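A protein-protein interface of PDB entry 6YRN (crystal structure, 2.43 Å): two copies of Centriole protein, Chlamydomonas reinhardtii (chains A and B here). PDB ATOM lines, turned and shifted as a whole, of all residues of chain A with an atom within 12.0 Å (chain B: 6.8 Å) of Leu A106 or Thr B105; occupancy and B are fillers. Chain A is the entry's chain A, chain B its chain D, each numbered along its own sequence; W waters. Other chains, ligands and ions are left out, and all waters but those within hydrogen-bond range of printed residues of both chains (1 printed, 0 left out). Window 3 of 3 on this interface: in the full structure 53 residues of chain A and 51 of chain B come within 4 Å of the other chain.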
ATOM      1  N   GLN A  97      11.823 -26.435  -3.186  1.00  0.00           N
ATOM      2  CA  GLN A  97      12.469 -26.075  -4.444  1.00  0.00           C
ATOM      3  C   GLN A  97      11.511 -25.260  -5.338  1.00  0.00           C
ATOM      4  O   GLN A  97      11.947 -24.290  -5.962  1.00  0.00           O
ATOM      5  CB  GLN A  97      13.045 -27.317  -5.160  1.00  0.00           C
ATOM      6  CG  GLN A  97      13.954 -26.985  -6.357  1.00  0.00           C
ATOM      7  CD  GLN A  97      15.079 -26.007  -6.066  1.00  0.00           C
ATOM      8  OE1 GLN A  97      15.969 -26.280  -5.262  1.00  0.00           O
ATOM      9  NE2 GLN A  97      15.064 -24.848  -6.721  1.00  0.00           N
ATOM     10  N   ARG A  98      10.211 -25.614  -5.355  1.00  0.00           N
ATOM     11  CA  ARG A  98       9.172 -24.876  -6.101  1.00  0.00           C
ATOM     12  C   ARG A  98       8.989 -23.493  -5.521  1.00  0.00           C
ATOM     13  O   ARG A  98       8.822 -22.530  -6.268  1.00  0.00           O
ATOM     14  CB  ARG A  98       7.840 -25.645  -6.130  1.00  0.00           C
ATOM     15  CG  ARG A  98       7.836 -26.736  -7.212  1.00  0.00           C
ATOM     16  CD  ARG A  98       6.475 -27.317  -7.539  1.00  0.00           C
ATOM     17  NE  ARG A  98       5.787 -27.938  -6.402  1.00  0.00           N
ATOM     18  CZ  ARG A  98       5.974 -29.187  -5.976  1.00  0.00           C
ATOM     19  NH1 ARG A  98       6.887 -29.964  -6.548  1.00  0.00           N
ATOM     20  NH2 ARG A  98       5.264 -29.660  -4.960  1.00  0.00           N
ATOM     21  N   CYS A  99       9.057 -23.389  -4.185  1.00  0.00           N
ATOM     22  CA  CYS A  99       8.966 -22.147  -3.401  1.00  0.00           C
ATOM     23  C   CYS A  99      10.064 -21.196  -3.792  1.00  0.00           C
ATOM     24  O   CYS A  99       9.792 -20.046  -4.127  1.00  0.00           O
ATOM     25  CB  CYS A  99       9.063 -22.462  -1.915  1.00  0.00           C
ATOM     26  SG  CYS A  99       7.482 -22.597  -1.083  1.00  0.00           S
ATOM     27  N   ALA A 100      11.317 -21.705  -3.747  1.00  0.00           N
ATOM     28  CA  ALA A 100      12.549 -21.005  -4.061  1.00  0.00           C
ATOM     29  C   ALA A 100      12.501 -20.445  -5.474  1.00  0.00           C
ATOM     30  O   ALA A 100      12.953 -19.324  -5.692  1.00  0.00           O
ATOM     31  CB  ALA A 100      13.740 -21.947  -3.901  1.00  0.00           C
ATOM     32  N   ASP A 101      11.928 -21.208  -6.424  1.00  0.00           N
ATOM     33  CA  ASP A 101      11.794 -20.806  -7.822  1.00  0.00           C
ATOM     34  C   ASP A 101      10.740 -19.704  -7.980  1.00  0.00           C
ATOM     35  O   ASP A 101      10.954 -18.768  -8.750  1.00  0.00           O
ATOM     36  CB  ASP A 101      11.484 -22.031  -8.702  1.00  0.00           C
ATOM     37  CG  ASP A 101      12.631 -23.037  -8.883  1.00  0.00           C
ATOM     38  OD1 ASP A 101      13.809 -22.665  -8.621  1.00  0.00           O
ATOM     39  OD2 ASP A 101      12.351 -24.192  -9.292  1.00  0.00           O
ATOM     40  N   LEU A 102       9.622 -19.787  -7.216  1.00  0.00           N
ATOM     41  CA  LEU A 102       8.585 -18.759  -7.236  1.00  0.00           C
ATOM     42  C   LEU A 102       9.101 -17.470  -6.568  1.00  0.00           C
ATOM     43  O   LEU A 102       8.808 -16.365  -7.021  1.00  0.00           O
ATOM     44  CB  LEU A 102       7.333 -19.245  -6.514  1.00  0.00           C
ATOM     45  CG  LEU A 102       6.451 -20.253  -7.249  1.00  0.00           C
ATOM     46  CD1 LEU A 102       5.540 -20.954  -6.275  1.00  0.00           C
ATOM     47  CD2 LEU A 102       5.651 -19.570  -8.392  1.00  0.00           C
ATOM     48  N   ARG A 103       9.922 -17.634  -5.524  1.00  0.00           N
ATOM     49  CA  ARG A 103      10.528 -16.546  -4.767  1.00  0.00           C
ATOM     50  C   ARG A 103      11.506 -15.746  -5.668  1.00  0.00           C
ATOM     51  O   ARG A 103      11.496 -14.525  -5.648  1.00  0.00           O
ATOM     52  CB  ARG A 103      11.186 -17.092  -3.481  1.00  0.00           C
ATOM     53  CG  ARG A 103      11.301 -16.028  -2.409  1.00  0.00           C
ATOM     54  CD  ARG A 103      11.641 -16.541  -1.033  1.00  0.00           C
ATOM     55  NE  ARG A 103      10.459 -17.009  -0.299  1.00  0.00           N
ATOM     56  CZ  ARG A 103       9.561 -16.225   0.310  1.00  0.00           C
ATOM     57  NH1 ARG A 103       9.665 -14.894   0.238  1.00  0.00           N
ATOM     58  NH2 ARG A 103       8.536 -16.763   0.961  1.00  0.00           N
ATOM     59  N   ASP A 104      12.267 -16.440  -6.517  1.00  0.00           N
ATOM     60  CA  ASP A 104      13.208 -15.844  -7.470  1.00  0.00           C
ATOM     61  C   ASP A 104      12.473 -15.088  -8.562  1.00  0.00           C
ATOM     62  O   ASP A 104      12.919 -13.995  -8.922  1.00  0.00           O
ATOM     63  CB  ASP A 104      14.137 -16.918  -8.083  1.00  0.00           C
ATOM     64  CG  ASP A 104      15.230 -17.449  -7.162  1.00  0.00           C
ATOM     65  OD1 ASP A 104      15.814 -16.643  -6.407  1.00  0.00           O
ATOM     66  OD2 ASP A 104      15.517 -18.673  -7.217  1.00  0.00           O
ATOM     67  N   THR A 105      11.349 -15.666  -9.082  1.00  0.00           N
ATOM     68  CA  THR A 105      10.516 -15.066 -10.129  1.00  0.00           C
ATOM     69  C   THR A 105       9.872 -13.786  -9.610  1.00  0.00           C
ATOM     70  O   THR A 105       9.792 -12.797 -10.346  1.00  0.00           O
ATOM     71  CB  THR A 105       9.468 -16.067 -10.647  1.00  0.00           C
ATOM     72  OG1 THR A 105      10.098 -17.277 -11.061  1.00  0.00           O
ATOM     73  CG2 THR A 105       8.674 -15.519 -11.812  1.00  0.00           C
ATOM     74  N   LEU A 106       9.420 -13.804  -8.345  1.00  0.00           N
ATOM     75  CA  LEU A 106       8.787 -12.659  -7.707  1.00  0.00           C
ATOM     76  C   LEU A 106       9.803 -11.539  -7.479  1.00  0.00           C
ATOM     77  O   LEU A 106       9.524 -10.388  -7.833  1.00  0.00           O
ATOM     78  CB  LEU A 106       8.077 -13.063  -6.394  1.00  0.00           C
ATOM     79  CG  LEU A 106       7.307 -11.947  -5.654  1.00  0.00           C
ATOM     80  CD1 LEU A 106       6.010 -11.555  -6.391  1.00  0.00           C
ATOM     81  CD2 LEU A 106       6.989 -12.357  -4.215  1.00  0.00           C
ATOM     82  N   ALA A 107      10.986 -11.882  -6.931  1.00  0.00           N
ATOM     83  CA  ALA A 107      12.067 -10.937  -6.674  1.00  0.00           C
ATOM     84  C   ALA A 107      12.537 -10.260  -7.972  1.00  0.00           C
ATOM     85  O   ALA A 107      12.856  -9.062  -7.960  1.00  0.00           O
ATOM     86  CB  ALA A 107      13.223 -11.638  -5.984  1.00  0.00           C
ATOM     87  N   SER A 108      12.520 -11.021  -9.095  1.00  0.00           N
ATOM     88  CA  SER A 108      12.912 -10.580 -10.443  1.00  0.00           C
ATOM     89  C   SER A 108      11.910  -9.551 -10.965  1.00  0.00           C
ATOM     90  O   SER A 108      12.324  -8.490 -11.445  1.00  0.00           O
ATOM     91  CB  SER A 108      13.019 -11.775 -11.399  1.00  0.00           C
ATOM     92  OG  SER A 108      13.572 -11.424 -12.656  1.00  0.00           O
ATOM     93  N   ALA A 109      10.589  -9.852 -10.825  1.00  0.00           N
ATOM     94  CA  ALA A 109       9.502  -8.969 -11.252  1.00  0.00           C
ATOM     95  C   ALA A 109       9.512  -7.656 -10.464  1.00  0.00           C
ATOM     96  O   ALA A 109       9.281  -6.591 -11.058  1.00  0.00           O
ATOM     97  CB  ALA A 109       8.164  -9.672 -11.111  1.00  0.00           C
ATOM     98  N   GLU A 110       9.818  -7.731  -9.139  1.00  0.00           N
ATOM     99  CA  GLU A 110       9.921  -6.573  -8.236  1.00  0.00           C
ATOM    100  C   GLU A 110      11.034  -5.624  -8.714  1.00  0.00           C
ATOM    101  O   GLU A 110      10.821  -4.416  -8.763  1.00  0.00           O
ATOM    102  CB  GLU A 110      10.195  -7.016  -6.785  1.00  0.00           C
ATOM    103  CG  GLU A 110       8.981  -7.559  -6.036  1.00  0.00           C
ATOM    104  CD  GLU A 110       9.238  -8.183  -4.669  1.00  0.00           C
ATOM    105  OE1 GLU A 110      10.378  -8.083  -4.157  1.00  0.00           O
ATOM    106  OE2 GLU A 110       8.293  -8.786  -4.112  1.00  0.00           O
ATOM    107  N   GLY A 111      12.181  -6.194  -9.085  1.00  0.00           N
ATOM    108  CA  GLY A 111      13.342  -5.467  -9.596  1.00  0.00           C
ATOM    109  C   GLY A 111      13.077  -4.779 -10.923  1.00  0.00           C
ATOM    110  O   GLY A 111      13.521  -3.644 -11.136  1.00  0.00           O
ATOM    111  N   ARG A 112      12.339  -5.481 -11.825  1.00  0.00           N
ATOM    112  CA  ARG A 112      11.903  -4.998 -13.143  1.00  0.00           C
ATOM    113  C   ARG A 112      10.929  -3.819 -12.964  1.00  0.00           C
ATOM    114  O   ARG A 112      11.088  -2.782 -13.602  1.00  0.00           O
ATOM    115  CB  ARG A 112      11.226  -6.131 -13.938  1.00  0.00           C
ATOM    116  CG  ARG A 112      12.203  -6.991 -14.746  1.00  0.00           C
ATOM    117  CD  ARG A 112      11.492  -8.183 -15.354  1.00  0.00           C
ATOM    118  NE  ARG A 112      12.398  -9.256 -15.770  1.00  0.00           N
ATOM    119  CZ  ARG A 112      11.997 -10.414 -16.293  1.00  0.00           C
ATOM    120  NH1 ARG A 112      10.704 -10.661 -16.466  1.00  0.00           N
ATOM    121  NH2 ARG A 112      12.888 -11.332 -16.654  1.00  0.00           N
ATOM    122  N   ALA A 113       9.945  -3.961 -12.067  1.00  0.00           N
ATOM    123  CA  ALA A 113       8.960  -2.913 -11.773  1.00  0.00           C
ATOM    124  C   ALA A 113       9.637  -1.626 -11.246  1.00  0.00           C
ATOM    125  O   ALA A 113       9.305  -0.525 -11.702  1.00  0.00           O
ATOM    126  CB  ALA A 113       7.944  -3.432 -10.770  1.00  0.00           C
ATOM    127  N   LYS A 114      10.630  -1.795 -10.337  1.00  0.00           N
ATOM    128  CA  LYS A 114      11.411  -0.726  -9.702  1.00  0.00           C
ATOM    129  C   LYS A 114      12.133   0.161 -10.714  1.00  0.00           C
ATOM    130  O   LYS A 114      12.039   1.390 -10.611  1.00  0.00           O
ATOM    131  CB  LYS A 114      12.403  -1.293  -8.667  1.00  0.00           C
ATOM    132  CG  LYS A 114      11.765  -1.631  -7.326  1.00  0.00           C
ATOM    133  CD  LYS A 114      12.718  -2.387  -6.413  1.00  0.00           C
ATOM    134  CE  LYS A 114      12.008  -2.996  -5.228  1.00  0.00           C
ATOM    135  NZ  LYS A 114      12.964  -3.532  -4.232  1.00  0.00           N
ATOM    136  N   GLU A 115      12.842  -0.450 -11.683  1.00  0.00           N
ATOM    137  CA  GLU A 115      13.579   0.285 -12.705  1.00  0.00           C
ATOM    138  C   GLU A 115      12.618   1.035 -13.674  1.00  0.00           C
ATOM    139  O   GLU A 115      12.932   2.166 -14.063  1.00  0.00           O
ATOM    140  CB  GLU A 115      14.585  -0.638 -13.406  1.00  0.00           C
ATOM    141  CG  GLU A 115      15.473   0.011 -14.457  1.00  0.00           C
ATOM    142  CD  GLU A 115      16.244  -0.983 -15.308  1.00  0.00           C
ATOM    143  OE1 GLU A 115      16.173  -2.193 -15.002  1.00  0.00           O
ATOM    144  OE2 GLU A 115      16.916  -0.560 -16.279  1.00  0.00           O
ATOM    145  N   ALA B 100       1.521 -21.676  -2.807  1.00  0.00           N
ATOM    146  CA  ALA B 100       0.223 -21.195  -3.246  1.00  0.00           C
ATOM    147  C   ALA B 100       0.098 -19.682  -3.050  1.00  0.00           C
ATOM    148  O   ALA B 100      -0.382 -19.003  -3.953  1.00  0.00           O
ATOM    149  CB  ALA B 100      -0.877 -21.936  -2.498  1.00  0.00           C
ATOM    150  N   ASP B 101       0.591 -19.163  -1.911  1.00  0.00           N
ATOM    151  CA  ASP B 101       0.614 -17.746  -1.594  1.00  0.00           C
ATOM    152  C   ASP B 101       1.606 -16.987  -2.474  1.00  0.00           C
ATOM    153  O   ASP B 101       1.299 -15.876  -2.881  1.00  0.00           O
ATOM    154  CB  ASP B 101       0.920 -17.523  -0.105  1.00  0.00           C
ATOM    155  CG  ASP B 101      -0.205 -17.899   0.862  1.00  0.00           C
ATOM    156  OD1 ASP B 101      -1.386 -18.012   0.409  1.00  0.00           O
ATOM    157  OD2 ASP B 101       0.083 -18.049   2.071  1.00  0.00           O
ATOM    158  N   LEU B 102       2.766 -17.594  -2.800  1.00  0.00           N
ATOM    159  CA  LEU B 102       3.760 -16.974  -3.686  1.00  0.00           C
ATOM    160  C   LEU B 102       3.231 -16.926  -5.108  1.00  0.00           C
ATOM    161  O   LEU B 102       3.444 -15.917  -5.765  1.00  0.00           O
ATOM    162  CB  LEU B 102       5.111 -17.696  -3.645  1.00  0.00           C
ATOM    163  CG  LEU B 102       5.990 -17.455  -2.416  1.00  0.00           C
ATOM    164  CD1 LEU B 102       7.043 -18.511  -2.304  1.00  0.00           C
ATOM    165  CD2 LEU B 102       6.642 -16.062  -2.432  1.00  0.00           C
ATOM    166  N   ARG B 103       2.473 -17.973  -5.547  1.00  0.00           N
ATOM    167  CA  ARG B 103       1.845 -18.059  -6.880  1.00  0.00           C
ATOM    168  C   ARG B 103       0.856 -16.912  -7.062  1.00  0.00           C
ATOM    169  O   ARG B 103       0.858 -16.258  -8.109  1.00  0.00           O
ATOM    170  CB  ARG B 103       1.114 -19.403  -7.085  1.00  0.00           C
ATOM    171  CG  ARG B 103       2.034 -20.553  -7.456  1.00  0.00           C
ATOM    172  CD  ARG B 103       1.349 -21.917  -7.450  1.00  0.00           C
ATOM    173  NE  ARG B 103       2.326 -23.000  -7.290  1.00  0.00           N
ATOM    174  CZ  ARG B 103       2.260 -23.980  -6.389  1.00  0.00           C
ATOM    175  NH1 ARG B 103       1.242 -24.037  -5.534  1.00  0.00           N
ATOM    176  NH2 ARG B 103       3.206 -24.902  -6.332  1.00  0.00           N
ATOM    177  N   ASP B 104       0.041 -16.653  -6.028  1.00  0.00           N
ATOM    178  CA  ASP B 104      -0.975 -15.599  -6.010  1.00  0.00           C
ATOM    179  C   ASP B 104      -0.364 -14.192  -6.043  1.00  0.00           C
ATOM    180  O   ASP B 104      -0.819 -13.340  -6.815  1.00  0.00           O
ATOM    181  CB  ASP B 104      -1.925 -15.795  -4.810  1.00  0.00           C
ATOM    182  CG  ASP B 104      -2.828 -17.029  -4.891  1.00  0.00           C
ATOM    183  OD1 ASP B 104      -3.292 -17.365  -6.013  1.00  0.00           O
ATOM    184  OD2 ASP B 104      -3.083 -17.652  -3.828  1.00  0.00           O
ATOM    185  N   THR B 105       0.700 -13.978  -5.244  1.00  0.00           N
ATOM    186  CA  THR B 105       1.454 -12.716  -5.170  1.00  0.00           C
ATOM    187  C   THR B 105       2.183 -12.475  -6.497  1.00  0.00           C
ATOM    188  O   THR B 105       2.274 -11.330  -6.929  1.00  0.00           O
ATOM    189  CB  THR B 105       2.433 -12.740  -3.986  1.00  0.00           C
ATOM    190  OG1 THR B 105       1.709 -12.994  -2.790  1.00  0.00           O
ATOM    191  CG2 THR B 105       3.196 -11.452  -3.819  1.00  0.00           C
ATOM    192  N   LEU B 106       2.684 -13.553  -7.141  1.00  0.00           N
ATOM    193  CA  LEU B 106       3.390 -13.473  -8.413  1.00  0.00           C
ATOM    194  C   LEU B 106       2.417 -13.083  -9.520  1.00  0.00           C
ATOM    195  O   LEU B 106       2.721 -12.150 -10.288  1.00  0.00           O
ATOM    196  CB  LEU B 106       4.132 -14.787  -8.740  1.00  0.00           C
ATOM    197  CG  LEU B 106       4.901 -14.847 -10.052  1.00  0.00           C
ATOM    198  CD1 LEU B 106       6.128 -13.911 -10.021  1.00  0.00           C
ATOM    199  CD2 LEU B 106       5.222 -16.293 -10.423  1.00  0.00           C
ATOM    200  N   ALA B 107       1.244 -13.765  -9.581  1.00  0.00           N
ATOM    201  CA  ALA B 107       0.200 -13.493 -10.564  1.00  0.00           C
ATOM    202  C   ALA B 107      -0.267 -12.025 -10.456  1.00  0.00           C
ATOM    203  O   ALA B 107      -0.491 -11.383 -11.481  1.00  0.00           O
ATOM    204  CB  ALA B 107      -0.967 -14.445 -10.360  1.00  0.00           C
ATOM    205  N   SER B 108      -0.352 -11.497  -9.210  1.00  0.00           N
ATOM    206  CA  SER B 108      -0.748 -10.129  -8.891  1.00  0.00           C
ATOM    207  C   SER B 108       0.281  -9.118  -9.431  1.00  0.00           C
ATOM    208  O   SER B 108      -0.106  -8.154 -10.104  1.00  0.00           O
ATOM    209  CB  SER B 108      -0.940  -9.973  -7.385  1.00  0.00           C
ATOM    210  OG  SER B 108      -1.546  -8.734  -7.061  1.00  0.00           O
ATOM    211  N   ALA B 109       1.584  -9.357  -9.156  1.00  0.00           N
ATOM    212  CA  ALA B 109       2.701  -8.510  -9.595  1.00  0.00           C
ATOM    213  C   ALA B 109       2.813  -8.473 -11.118  1.00  0.00           C
ATOM    214  O   ALA B 109       3.110  -7.416 -11.676  1.00  0.00           O
ATOM    215  CB  ALA B 109       4.007  -8.987  -8.978  1.00  0.00           C
ATOM    216  N   GLU B 110       2.550  -9.625 -11.783  1.00  0.00           N
ATOM    217  CA  GLU B 110       2.558  -9.763 -13.243  1.00  0.00           C
ATOM    218  C   GLU B 110       1.469  -8.879 -13.848  1.00  0.00           C
ATOM    219  O   GLU B 110       1.734  -8.178 -14.828  1.00  0.00           O
ATOM    220  CB  GLU B 110       2.328 -11.226 -13.656  1.00  0.00           C
ATOM    221  CG  GLU B 110       3.554 -12.114 -13.559  1.00  0.00           C
ATOM    222  CD  GLU B 110       3.338 -13.598 -13.823  1.00  0.00           C
ATOM    223  OE1 GLU B 110       2.223 -14.004 -14.228  1.00  0.00           O
ATOM    224  OE2 GLU B 110       4.308 -14.363 -13.621  1.00  0.00           O
ATOM    225  N   ARG B 112      -0.053  -6.214 -12.412  1.00  0.00           N
ATOM    226  CA  ARG B 112       0.267  -4.798 -12.162  1.00  0.00           C
ATOM    227  C   ARG B 112       1.323  -4.298 -13.155  1.00  0.00           C
ATOM    228  O   ARG B 112       1.190  -3.176 -13.659  1.00  0.00           O
ATOM    229  CB  ARG B 112       0.758  -4.570 -10.728  1.00  0.00           C
ATOM    230  CG  ARG B 112      -0.345  -4.572  -9.664  1.00  0.00           C
ATOM    231  CD  ARG B 112       0.158  -4.096  -8.297  1.00  0.00           C
ATOM    232  NE  ARG B 112       1.338  -4.838  -7.830  1.00  0.00           N
ATOM    233  CZ  ARG B 112       1.291  -5.958  -7.107  1.00  0.00           C
ATOM    234  NH1 ARG B 112       0.126  -6.473  -6.735  1.00  0.00           N
ATOM    235  NH2 ARG B 112       2.417  -6.556  -6.728  1.00  0.00           N
HETATM  236  O   HOH W   1       3.886 -26.541  -4.299  1.00  0.00           O
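Water W1 bridges the guanidinium group of Arg B103 (2.7 Å) and the guanidinium group of Arg A98 (3.2 Å).
Of the printed residues of chain B, Arg A103 touches Leu B102 (3.9 Å). Printed residues of chain B within 4 Å of Thr A105: Leu B106 (3.5 Å). Leu A106 touches just these residues of chain B: Thr B105 and Leu B106. No residue of chain A comes within 4 Å of Asp B101. Leu B102 touches just these residues of chain A: Cys A99 (3.6 Å), Leu A102 (3.9 Å) and Arg A103 (3.9 Å). No residue of chain A comes within 4 Å of Asp B104. Thr B105 touches one residue of chain A. No residue of chain A comes within 4 Å of Ala B107. Ala B109 touches none of the printed residues of chain A. The nearest residue of chain B that does not touch Leu A106 is Leu B102 (4.1 Å). The nearest residue of chain A that does not touch Thr B105 is Glu A110 (5.8 Å).
O of Asp B101 is in hydrogen-bond range of OG1 of Thr B105. The side-chain hydroxyl of Thr A105 lies within hydrogen-bond range of the backbone carbonyl oxygen of Asp A101.
Leu A102 touches its own counterpart, Leu B102. Leu A102 touches Leu B106, but with the chains exchanged Leu A106 does not touch Leu B102 (4.1 Å). Thr A105 touches Leu B106, and with the chains exchanged Leu A106 touches Thr B105. Leu A106 touches its own counterpart, Leu B106.
Of the 12 printed residues of chain B, 4 touch a printed residue of chain A. Printed residues of chain B that touch a printed residue of chain A: Leu B102, Arg B103, Thr B105 and Leu B106. Of the 19 printed residues of chain A, 6 touch a printed residue of chain B. Hydrophobic or aromatic side chains of chain A that line the printed part of chain B: Leu A102 and Leu A106. Among the printed residues, 9 pairs touch across the chains.
Among the printed residues, pairs that only touch across the chains: Arg A98 with Arg B103 (3.99 Å), Cys A99 with Leu B102 (3.6 Å), Leu A102 with Leu B102 (3.9 Å), Leu A102 with Arg B103 (3.7 Å), Leu A102 with Leu B106 (3.9 Å), Arg A103 with Leu B102 (3.9 Å), Thr A105 with Leu B106 (3.5 Å), Leu A106 with Thr B105 (3.8 Å) and Leu A106 with Leu B106 (3.7 Å).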
